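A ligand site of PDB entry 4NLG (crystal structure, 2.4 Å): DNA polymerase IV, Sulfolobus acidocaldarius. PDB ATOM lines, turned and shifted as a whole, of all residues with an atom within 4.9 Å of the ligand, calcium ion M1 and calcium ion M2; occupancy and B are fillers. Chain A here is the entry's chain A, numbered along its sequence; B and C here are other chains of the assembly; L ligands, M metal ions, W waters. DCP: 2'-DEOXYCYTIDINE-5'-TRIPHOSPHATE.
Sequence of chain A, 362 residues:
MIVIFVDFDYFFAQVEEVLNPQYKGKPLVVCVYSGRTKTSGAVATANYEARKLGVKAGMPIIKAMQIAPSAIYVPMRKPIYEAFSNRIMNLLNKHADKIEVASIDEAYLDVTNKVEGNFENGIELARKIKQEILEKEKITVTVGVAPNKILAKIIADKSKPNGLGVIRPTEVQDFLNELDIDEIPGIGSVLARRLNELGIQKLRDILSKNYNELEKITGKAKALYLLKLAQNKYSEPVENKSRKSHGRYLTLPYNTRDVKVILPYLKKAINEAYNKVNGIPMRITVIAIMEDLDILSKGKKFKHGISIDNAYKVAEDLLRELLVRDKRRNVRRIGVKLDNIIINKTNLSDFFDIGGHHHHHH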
ATOM      1  N   ASP A   7      28.935 -19.128 -36.510  1.00  0.00           N
ATOM      2  CA  ASP A   7      28.032 -18.606 -35.504  1.00  0.00           C
ATOM      3  C   ASP A   7      26.801 -18.138 -36.274  1.00  0.00           C
ATOM      4  O   ASP A   7      26.933 -17.313 -37.174  1.00  0.00           O
ATOM      5  CB  ASP A   7      28.714 -17.476 -34.720  1.00  0.00           C
ATOM      6  CG  ASP A   7      28.010 -17.165 -33.382  1.00  0.00           C
ATOM      7  OD1 ASP A   7      26.862 -17.629 -33.153  1.00  0.00           O
ATOM      8  OD2 ASP A   7      28.621 -16.471 -32.538  1.00  0.00           O
ATOM      9  N   PHE A   8      25.621 -18.692 -35.971  1.00  0.00           N
ATOM     10  CA  PHE A   8      24.407 -18.356 -36.724  1.00  0.00           C
ATOM     11  C   PHE A   8      23.960 -16.931 -36.349  1.00  0.00           C
ATOM     12  O   PHE A   8      24.099 -16.545 -35.202  1.00  0.00           O
ATOM     13  CB  PHE A   8      23.282 -19.371 -36.462  1.00  0.00           C
ATOM     14  CG  PHE A   8      23.711 -20.817 -36.535  1.00  0.00           C
ATOM     15  CD1 PHE A   8      22.991 -21.789 -35.867  1.00  0.00           C
ATOM     16  CD2 PHE A   8      24.815 -21.205 -37.301  1.00  0.00           C
ATOM     17  CE1 PHE A   8      23.377 -23.139 -35.932  1.00  0.00           C
ATOM     18  CE2 PHE A   8      25.189 -22.540 -37.378  1.00  0.00           C
ATOM     19  CZ  PHE A   8      24.471 -23.502 -36.676  1.00  0.00           C
ATOM     20  N   ASP A   9      23.447 -16.146 -37.302  1.00  0.00           N
ATOM     21  CA  ASP A   9      23.083 -14.728 -37.016  1.00  0.00           C
ATOM     22  C   ASP A   9      21.741 -14.637 -36.274  1.00  0.00           C
ATOM     23  O   ASP A   9      20.829 -15.398 -36.582  1.00  0.00           O
ATOM     24  CB  ASP A   9      23.019 -13.902 -38.303  1.00  0.00           C
ATOM     25  CG  ASP A   9      24.389 -13.731 -38.960  1.00  0.00           C
ATOM     26  OD1 ASP A   9      24.437 -13.742 -40.210  1.00  0.00           O
ATOM     27  OD2 ASP A   9      25.402 -13.588 -38.242  1.00  0.00           O
ATOM     28  N   TYR A  10      21.635 -13.710 -35.314  1.00  0.00           N
ATOM     29  CA  TYR A  10      20.442 -13.549 -34.465  1.00  0.00           C
ATOM     30  C   TYR A  10      19.552 -14.813 -34.487  1.00  0.00           C
ATOM     31  O   TYR A  10      18.365 -14.779 -34.860  1.00  0.00           O
ATOM     32  CB  TYR A  10      19.670 -12.280 -34.884  1.00  0.00           C
ATOM     33  CG  TYR A  10      19.131 -12.246 -36.307  1.00  0.00           C
ATOM     34  CD1 TYR A  10      17.751 -12.262 -36.542  1.00  0.00           C
ATOM     35  CD2 TYR A  10      19.982 -12.189 -37.407  1.00  0.00           C
ATOM     36  CE1 TYR A  10      17.239 -12.255 -37.860  1.00  0.00           C
ATOM     37  CE2 TYR A  10      19.489 -12.190 -38.735  1.00  0.00           C
ATOM     38  CZ  TYR A  10      18.118 -12.218 -38.945  1.00  0.00           C
ATOM     39  OH  TYR A  10      17.613 -12.190 -40.237  1.00  0.00           O
ATOM     40  N   PHE A  11      20.153 -15.937 -34.082  1.00  0.00           N
ATOM     41  CA  PHE A  11      19.671 -17.270 -34.470  1.00  0.00           C
ATOM     42  C   PHE A  11      18.207 -17.556 -34.187  1.00  0.00           C
ATOM     43  O   PHE A  11      17.444 -17.814 -35.122  1.00  0.00           O
ATOM     44  CB  PHE A  11      20.534 -18.350 -33.796  1.00  0.00           C
ATOM     45  CG  PHE A  11      20.121 -19.774 -34.161  1.00  0.00           C
ATOM     46  CD1 PHE A  11      19.949 -20.143 -35.484  1.00  0.00           C
ATOM     47  CD2 PHE A  11      19.946 -20.743 -33.175  1.00  0.00           C
ATOM     48  CE1 PHE A  11      19.579 -21.476 -35.850  1.00  0.00           C
ATOM     49  CE2 PHE A  11      19.587 -22.068 -33.526  1.00  0.00           C
ATOM     50  CZ  PHE A  11      19.395 -22.424 -34.855  1.00  0.00           C
ATOM     51  N   PHE A  12      17.782 -17.549 -32.916  1.00  0.00           N
ATOM     52  CA  PHE A  12      16.363 -17.855 -32.645  1.00  0.00           C
ATOM     53  C   PHE A  12      15.426 -16.906 -33.424  1.00  0.00           C
ATOM     54  O   PHE A  12      14.417 -17.359 -33.962  1.00  0.00           O
ATOM     55  CB  PHE A  12      16.045 -17.782 -31.148  1.00  0.00           C
ATOM     56  CG  PHE A  12      16.804 -18.790 -30.322  1.00  0.00           C
ATOM     57  CD1 PHE A  12      17.783 -19.592 -30.887  1.00  0.00           C
ATOM     58  CD2 PHE A  12      16.518 -18.950 -28.957  1.00  0.00           C
ATOM     59  CE1 PHE A  12      18.477 -20.532 -30.130  1.00  0.00           C
ATOM     60  CE2 PHE A  12      17.211 -19.868 -28.197  1.00  0.00           C
ATOM     61  CZ  PHE A  12      18.177 -20.672 -28.794  1.00  0.00           C
ATOM     62  N   VAL A  43      14.289 -11.422 -22.642  1.00  0.00           N
ATOM     63  CA  VAL A  43      14.472 -11.488 -24.065  1.00  0.00           C
ATOM     64  C   VAL A  43      15.505 -12.576 -24.309  1.00  0.00           C
ATOM     65  O   VAL A  43      16.520 -12.624 -23.613  1.00  0.00           O
ATOM     66  CB  VAL A  43      14.946 -10.140 -24.647  1.00  0.00           C
ATOM     67  CG1 VAL A  43      15.434 -10.319 -26.068  1.00  0.00           C
ATOM     68  CG2 VAL A  43      13.807  -9.105 -24.582  1.00  0.00           C
ATOM     69  N   ALA A  44      15.274 -13.446 -25.272  1.00  0.00           N
ATOM     70  CA  ALA A  44      16.299 -14.437 -25.590  1.00  0.00           C
ATOM     71  C   ALA A  44      17.158 -13.880 -26.708  1.00  0.00           C
ATOM     72  O   ALA A  44      18.395 -13.917 -26.649  1.00  0.00           O
ATOM     73  CB  ALA A  44      15.667 -15.792 -25.987  1.00  0.00           C
ATOM     74  N   THR A  45      16.494 -13.375 -27.736  1.00  0.00           N
ATOM     75  CA  THR A  45      17.168 -12.764 -28.862  1.00  0.00           C
ATOM     76  C   THR A  45      16.242 -11.785 -29.625  1.00  0.00           C
ATOM     77  O   THR A  45      15.018 -11.933 -29.661  1.00  0.00           O
ATOM     78  CB  THR A  45      17.737 -13.852 -29.794  1.00  0.00           C
ATOM     79  OG1 THR A  45      18.443 -13.252 -30.884  1.00  0.00           O
ATOM     80  CG2 THR A  45      16.649 -14.734 -30.326  1.00  0.00           C
ATOM     81  N   TYR A  48      18.073  -7.705 -35.839  1.00  0.00           N
ATOM     82  CA  TYR A  48      18.889  -6.504 -35.835  1.00  0.00           C
ATOM     83  C   TYR A  48      18.055  -5.210 -35.887  1.00  0.00           C
ATOM     84  O   TYR A  48      18.474  -4.160 -35.378  1.00  0.00           O
ATOM     85  CB  TYR A  48      19.895  -6.576 -37.001  1.00  0.00           C
ATOM     86  CG  TYR A  48      21.090  -7.425 -36.618  1.00  0.00           C
ATOM     87  CD1 TYR A  48      22.193  -6.871 -35.988  1.00  0.00           C
ATOM     88  CD2 TYR A  48      21.087  -8.797 -36.834  1.00  0.00           C
ATOM     89  CE1 TYR A  48      23.283  -7.637 -35.609  1.00  0.00           C
ATOM     90  CE2 TYR A  48      22.169  -9.580 -36.467  1.00  0.00           C
ATOM     91  CZ  TYR A  48      23.256  -9.003 -35.852  1.00  0.00           C
ATOM     92  OH  TYR A  48      24.341  -9.772 -35.480  1.00  0.00           O
ATOM     93  N   ARG A  51      17.397  -4.590 -32.373  1.00  0.00           N
ATOM     94  CA  ARG A  51      18.581  -4.124 -31.689  1.00  0.00           C
ATOM     95  C   ARG A  51      18.790  -2.617 -31.958  1.00  0.00           C
ATOM     96  O   ARG A  51      19.307  -1.918 -31.099  1.00  0.00           O
ATOM     97  CB  ARG A  51      19.816  -4.938 -32.063  1.00  0.00           C
ATOM     98  CG  ARG A  51      19.698  -6.404 -31.681  1.00  0.00           C
ATOM     99  CD  ARG A  51      20.936  -7.235 -32.006  1.00  0.00           C
ATOM    100  NE  ARG A  51      20.640  -8.662 -31.893  1.00  0.00           N
ATOM    101  CZ  ARG A  51      21.527  -9.646 -32.093  1.00  0.00           C
ATOM    102  NH1 ARG A  51      22.785  -9.345 -32.416  1.00  0.00           N
ATOM    103  NH2 ARG A  51      21.153 -10.923 -31.974  1.00  0.00           N
ATOM    104  N   ALA A  57      19.668  -9.073 -25.577  1.00  0.00           N
ATOM    105  CA  ALA A  57      19.423 -10.373 -24.951  1.00  0.00           C
ATOM    106  C   ALA A  57      19.590 -10.229 -23.445  1.00  0.00           C
ATOM    107  O   ALA A  57      20.453  -9.488 -22.949  1.00  0.00           O
ATOM    108  CB  ALA A  57      20.340 -11.444 -25.501  1.00  0.00           C
ATOM    109  N   GLY A  58      18.736 -10.923 -22.713  1.00  0.00           N
ATOM    110  CA  GLY A  58      18.800 -10.919 -21.270  1.00  0.00           C
ATOM    111  C   GLY A  58      17.935  -9.861 -20.629  1.00  0.00           C
ATOM    112  O   GLY A  58      17.707  -9.888 -19.411  1.00  0.00           O
ATOM    113  N   SER A 103      27.849 -24.920 -28.990  1.00  0.00           N
ATOM    114  CA  SER A 103      26.586 -24.477 -28.420  1.00  0.00           C
ATOM    115  C   SER A 103      25.501 -24.594 -29.469  1.00  0.00           C
ATOM    116  O   SER A 103      25.730 -25.091 -30.568  1.00  0.00           O
ATOM    117  CB  SER A 103      26.671 -23.022 -27.925  1.00  0.00           C
ATOM    118  OG  SER A 103      26.526 -22.111 -29.001  1.00  0.00           O
ATOM    119  N   ILE A 104      24.312 -24.107 -29.147  1.00  0.00           N
ATOM    120  CA  ILE A 104      23.210 -24.393 -30.035  1.00  0.00           C
ATOM    121  C   ILE A 104      23.415 -23.659 -31.358  1.00  0.00           C
ATOM    122  O   ILE A 104      22.849 -24.051 -32.389  1.00  0.00           O
ATOM    123  CB  ILE A 104      21.862 -24.042 -29.376  1.00  0.00           C
ATOM    124  CG1 ILE A 104      20.688 -24.598 -30.199  1.00  0.00           C
ATOM    125  CG2 ILE A 104      21.737 -22.529 -29.122  1.00  0.00           C
ATOM    126  CD1 ILE A 104      19.362 -24.375 -29.514  1.00  0.00           C
ATOM    127  N   ASP A 105      24.271 -22.648 -31.379  1.00  0.00           N
ATOM    128  CA  ASP A 105      24.369 -21.846 -32.601  1.00  0.00           C
ATOM    129  C   ASP A 105      25.806 -21.598 -33.062  1.00  0.00           C
ATOM    130  O   ASP A 105      26.074 -20.727 -33.887  1.00  0.00           O
ATOM    131  CB  ASP A 105      23.578 -20.522 -32.398  1.00  0.00           C
ATOM    132  CG  ASP A 105      24.477 -19.309 -32.216  1.00  0.00           C
ATOM    133  OD1 ASP A 105      25.437 -19.322 -31.441  1.00  0.00           O
ATOM    134  OD2 ASP A 105      24.180 -18.317 -32.886  1.00  0.00           O
ATOM    135  N   GLU A 106      26.746 -22.384 -32.568  1.00  0.00           N
ATOM    136  CA  GLU A 106      28.106 -22.218 -33.035  1.00  0.00           C
ATOM    137  C   GLU A 106      28.972 -23.498 -32.974  1.00  0.00           C
ATOM    138  O   GLU A 106      28.796 -24.361 -32.116  1.00  0.00           O
ATOM    139  CB  GLU A 106      28.774 -21.090 -32.238  1.00  0.00           C
ATOM    140  CG  GLU A 106      28.751 -21.274 -30.736  1.00  0.00           C
ATOM    141  CD  GLU A 106      29.199 -20.031 -29.996  1.00  0.00           C
ATOM    142  OE1 GLU A 106      29.818 -19.160 -30.625  1.00  0.00           O
ATOM    143  OE2 GLU A 106      28.917 -19.905 -28.790  1.00  0.00           O
ATOM    144  N   LYS A 160      30.459 -10.058 -37.596  1.00  0.00           N
ATOM    145  CA  LYS A 160      28.998 -10.110 -37.542  1.00  0.00           C
ATOM    146  C   LYS A 160      28.403  -8.782 -38.008  1.00  0.00           C
ATOM    147  O   LYS A 160      29.038  -7.732 -37.849  1.00  0.00           O
ATOM    148  CB  LYS A 160      28.500 -10.404 -36.119  1.00  0.00           C
ATOM    149  CG  LYS A 160      29.026 -11.691 -35.497  1.00  0.00           C
ATOM    150  CD  LYS A 160      28.357 -11.939 -34.130  1.00  0.00           C
ATOM    151  CE  LYS A 160      28.817 -13.258 -33.465  1.00  0.00           C
ATOM    152  NZ  LYS A 160      27.935 -13.655 -32.292  1.00  0.00           N
ATOM    153  P    DG B   5      10.948 -13.925 -14.803  1.00  0.00           P
ATOM    154  OP1  DG B   5       9.494 -13.801 -14.517  1.00  0.00           O
ATOM    155  OP2  DG B   5      11.866 -14.430 -13.739  1.00  0.00           O
ATOM    156  O5'  DG B   5      11.131 -14.919 -16.023  1.00  0.00           O
ATOM    157  C5'  DG B   5      12.390 -15.003 -16.675  1.00  0.00           C
ATOM    158  C4'  DG B   5      12.366 -16.232 -17.534  1.00  0.00           C
ATOM    159  O4'  DG B   5      13.366 -16.182 -18.568  1.00  0.00           O
ATOM    160  C3'  DG B   5      12.613 -17.500 -16.773  1.00  0.00           C
ATOM    161  O3'  DG B   5      11.832 -18.486 -17.392  1.00  0.00           O
ATOM    162  C2'  DG B   5      14.137 -17.709 -16.942  1.00  0.00           C
ATOM    163  C1'  DG B   5      14.376 -17.160 -18.343  1.00  0.00           C
ATOM    164  N9   DG B   5      15.632 -16.456 -18.552  1.00  0.00           N
ATOM    165  C8   DG B   5      16.169 -15.491 -17.744  1.00  0.00           C
ATOM    166  N7   DG B   5      17.242 -14.939 -18.237  1.00  0.00           N
ATOM    167  C5   DG B   5      17.406 -15.547 -19.459  1.00  0.00           C
ATOM    168  C6   DG B   5      18.402 -15.351 -20.431  1.00  0.00           C
ATOM    169  O6   DG B   5      19.377 -14.577 -20.389  1.00  0.00           O
ATOM    170  N1   DG B   5      18.206 -16.170 -21.532  1.00  0.00           N
ATOM    171  C2   DG B   5      17.175 -17.067 -21.672  1.00  0.00           C
ATOM    172  N2   DG B   5      17.159 -17.775 -22.795  1.00  0.00           N
ATOM    173  N3   DG B   5      16.234 -17.260 -20.758  1.00  0.00           N
ATOM    174  C4   DG B   5      16.422 -16.475 -19.688  1.00  0.00           C
ATOM    175  P    DC B   6      11.787 -19.977 -16.833  1.00  0.00           P
ATOM    176  OP1  DC B   6      10.591 -20.533 -17.513  1.00  0.00           O
ATOM    177  OP2  DC B   6      11.861 -20.026 -15.355  1.00  0.00           O
ATOM    178  O5'  DC B   6      13.024 -20.634 -17.556  1.00  0.00           O
ATOM    179  C5'  DC B   6      12.901 -20.944 -18.923  1.00  0.00           C
ATOM    180  C4'  DC B   6      14.186 -21.514 -19.469  1.00  0.00           C
ATOM    181  O4'  DC B   6      15.208 -20.486 -19.477  1.00  0.00           O
ATOM    182  C3'  DC B   6      14.773 -22.703 -18.685  1.00  0.00           C
ATOM    183  O3'  DC B   6      15.128 -23.680 -19.621  1.00  0.00           O
ATOM    184  C2'  DC B   6      16.025 -22.105 -18.043  1.00  0.00           C
ATOM    185  C1'  DC B   6      16.418 -21.120 -19.126  1.00  0.00           C
ATOM    186  N1   DC B   6      17.390 -20.059 -18.753  1.00  0.00           N
ATOM    187  C2   DC B   6      18.359 -19.709 -19.691  1.00  0.00           C
ATOM    188  O2   DC B   6      18.365 -20.300 -20.771  1.00  0.00           O
ATOM    189  N3   DC B   6      19.245 -18.727 -19.416  1.00  0.00           N
ATOM    190  C4   DC B   6      19.183 -18.101 -18.256  1.00  0.00           C
ATOM    191  N4   DC B   6      20.077 -17.130 -18.035  1.00  0.00           N
ATOM    192  C5   DC B   6      18.200 -18.438 -17.257  1.00  0.00           C
ATOM    193  C6   DC B   6      17.326 -19.410 -17.548  1.00  0.00           C
ATOM    194  P    DG C  13      29.985 -16.445 -25.223  1.00  0.00           P
ATOM    195  OP1  DG C  13      31.120 -16.906 -26.056  1.00  0.00           O
ATOM    196  OP2  DG C  13      29.751 -15.005 -24.982  1.00  0.00           O
ATOM    197  O5'  DG C  13      28.642 -17.050 -25.817  1.00  0.00           O
ATOM    198  C5'  DG C  13      28.403 -18.435 -25.785  1.00  0.00           C
ATOM    199  C4'  DG C  13      26.940 -18.698 -26.057  1.00  0.00           C
ATOM    200  O4'  DG C  13      26.199 -18.558 -24.817  1.00  0.00           O
ATOM    201  C3'  DG C  13      26.322 -17.703 -27.028  1.00  0.00           C
ATOM    202  O3'  DG C  13      26.072 -18.346 -28.294  1.00  0.00           O
ATOM    203  C2'  DG C  13      25.025 -17.190 -26.318  1.00  0.00           C
ATOM    204  C1'  DG C  13      24.901 -18.109 -25.095  1.00  0.00           C
ATOM    205  N9   DG C  13      24.391 -17.463 -23.857  1.00  0.00           N
ATOM    206  C8   DG C  13      24.932 -16.362 -23.196  1.00  0.00           C
ATOM    207  N7   DG C  13      24.270 -16.020 -22.115  1.00  0.00           N
ATOM    208  C5   DG C  13      23.238 -16.972 -22.016  1.00  0.00           C
ATOM    209  C6   DG C  13      22.214 -17.133 -21.041  1.00  0.00           C
ATOM    210  O6   DG C  13      21.997 -16.448 -20.027  1.00  0.00           O
ATOM    211  N1   DG C  13      21.368 -18.203 -21.328  1.00  0.00           N
ATOM    212  C2   DG C  13      21.493 -19.038 -22.409  1.00  0.00           C
ATOM    213  N2   DG C  13      20.557 -19.993 -22.522  1.00  0.00           N
ATOM    214  N3   DG C  13      22.451 -18.909 -23.342  1.00  0.00           N
ATOM    215  C4   DG C  13      23.290 -17.859 -23.081  1.00  0.00           C
HETATM  216  N1  DCP L   1      20.560 -16.945 -25.906  1.00  0.00           N
HETATM  217  C2  DCP L   1      19.716 -16.928 -24.865  1.00  0.00           C
HETATM  218  N3  DCP L   1      19.827 -16.091 -23.832  1.00  0.00           N
HETATM  219  C4  DCP L   1      20.816 -15.207 -23.805  1.00  0.00           C
HETATM  220  C5  DCP L   1      21.727 -15.158 -24.851  1.00  0.00           C
HETATM  221  C6  DCP L   1      21.580 -16.054 -25.935  1.00  0.00           C
HETATM  222  O2  DCP L   1      18.697 -17.799 -24.848  1.00  0.00           O
HETATM  223  N4  DCP L   1      20.919 -14.344 -22.668  1.00  0.00           N
HETATM  224  C1' DCP L   1      20.317 -17.903 -27.018  1.00  0.00           C
HETATM  225  C2' DCP L   1      19.527 -17.197 -28.029  1.00  0.00           C
HETATM  226  C3' DCP L   1      20.531 -16.752 -29.020  1.00  0.00           C
HETATM  227  C4' DCP L   1      21.412 -17.869 -29.060  1.00  0.00           C
HETATM  228  O4' DCP L   1      21.467 -18.332 -27.674  1.00  0.00           O
HETATM  229  O3' DCP L   1      19.919 -16.524 -30.242  1.00  0.00           O
HETATM  230  C5' DCP L   1      22.722 -17.509 -29.593  1.00  0.00           C
HETATM  231  O5' DCP L   1      23.425 -16.531 -28.867  1.00  0.00           O
HETATM  232  PA  DCP L   1      24.266 -15.443 -29.624  1.00  0.00           P
HETATM  233  O1A DCP L   1      25.237 -14.800 -28.703  1.00  0.00           O
HETATM  234  O2A DCP L   1      25.096 -15.992 -30.751  1.00  0.00           O
HETATM  235  O3A DCP L   1      23.340 -14.296 -30.132  1.00  0.00           O
HETATM  236  PB  DCP L   1      22.570 -14.257 -31.486  1.00  0.00           P
HETATM  237  O1B DCP L   1      21.106 -14.361 -31.179  1.00  0.00           O
HETATM  238  O2B DCP L   1      22.691 -15.472 -32.358  1.00  0.00           O
HETATM  239  O3B DCP L   1      22.967 -12.940 -32.241  1.00  0.00           O
HETATM  240  PG  DCP L   1      24.350 -12.716 -32.924  1.00  0.00           P
HETATM  241  O1G DCP L   1      24.081 -12.362 -34.359  1.00  0.00           O
HETATM  242  O2G DCP L   1      25.066 -11.518 -32.369  1.00  0.00           O
HETATM  243  O3G DCP L   1      25.292 -13.954 -32.766  1.00  0.00           O
HETATM  244 CA    CA M   1      27.055 -17.637 -30.643  1.00  0.00          CA
HETATM  245 CA    CA M   2      24.890 -16.113 -33.153  1.00  0.00          CA
HETATM  246  O   HOH W   1      28.268 -15.868 -29.629  1.00  0.00           O
HETATM  247  O   HOH W   2      18.573 -20.707 -24.851  1.00  0.00           O
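Calcium ion M2 is bound by an oxygen (O3G) of the ligand (2.2 Å), the backbone carbonyl oxygen (O) of Phe 8 (2.2 Å), the side-chain carboxylate (OD2) of Asp 105 (2.3 Å), an oxygen (O2A) of the ligand (2.4 Å), an oxygen (O2B) of the ligand (2.4 Å) and the side-chain carboxylate (OD1) of Asp 7 (2.5 Å). Calcium ion M2 has six donor atoms within binding distance.
Of the 21 residues printed, 3 come within 4 Å of calcium ion M2.
OE2 of Glu 106 sits close to OG of Ser 103, 3.3 Å away. The side-chain hydroxyl (OH) of Tyr 48 lies within hydrogen-bond range of the guanidinium group (NH1) of Arg 51 (3.5 Å). The side-chain carboxylate of Asp 7 sits close to the side-chain amino group of Lys 160 (2.9 Å). OG of Ser 103 lies close to N of Asp 105, at 3.3 Å.
Water W1 lies within hydrogen-bond range of O1A of the ligand (3.3 Å) and NZ of Lys 160 (3.5 Å). Water W2 lies within hydrogen-bond range of an oxygen (O2) of the ligand (2.9 Å) and N2 of DG 13 of chain C (3.1 Å).
Calcium ion M1 is bound by water W1 (2.4 Å), the side-chain carboxylate (OD1) of Asp 105 (2.5 Å), the side-chain carboxylate (OD1) of Asp 7 (2.5 Å), an oxygen (O2A) of the ligand (2.6 Å), O3' of DG 13 of chain C (2.6 Å) and the side-chain carboxylate (OD2) of Asp 7 (2.7 Å). Calcium ion M1 has six donor atoms within binding distance.
Merely in contact with the ligand: Phe 12, Asp 9 and Ala 44. 14 residues have an atom within 4 Å of the ligand: Asp 7, Phe 8, Asp 9, Tyr 10, Phe 11, Phe 12, Ala 44, Thr 45, Tyr 48, Arg 51, Asp 105, Lys 160, DG 5 of chain B and DG 13 of chain C. The nearest printed residue that does not touch the ligand is Ala 57 (4.02 Å).
Glu 106 touches calcium ion M1.
The side-chain amino group (NZ) of Lys 160 lies within salt-bridge range of an oxygen (O2G) of the ligand, 3.6 Å away. An oxygen (O1G) of the ligand sits at hydrogen-bond distance from the backbone NH of Tyr 10 (3.0 Å). O1B of the ligand lies within hydrogen-bond range of OG1 of Thr 45. The backbone NH (N) of Phe 11 is in hydrogen-bond range of an oxygen (O1B) of the ligand (3.4 Å). An oxygen (O1G) of the ligand sits at hydrogen-bond distance from the side-chain hydroxyl (OH) of Tyr 48 (2.8 Å). An oxygen (O2G) of the ligand is in salt-bridge range of the guanidinium group of Arg 51 (3.2 Å). O6 of DG 5 of chain B is in hydrogen-bond range of a nitrogen (N4) of the ligand, at 2.8 Å.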
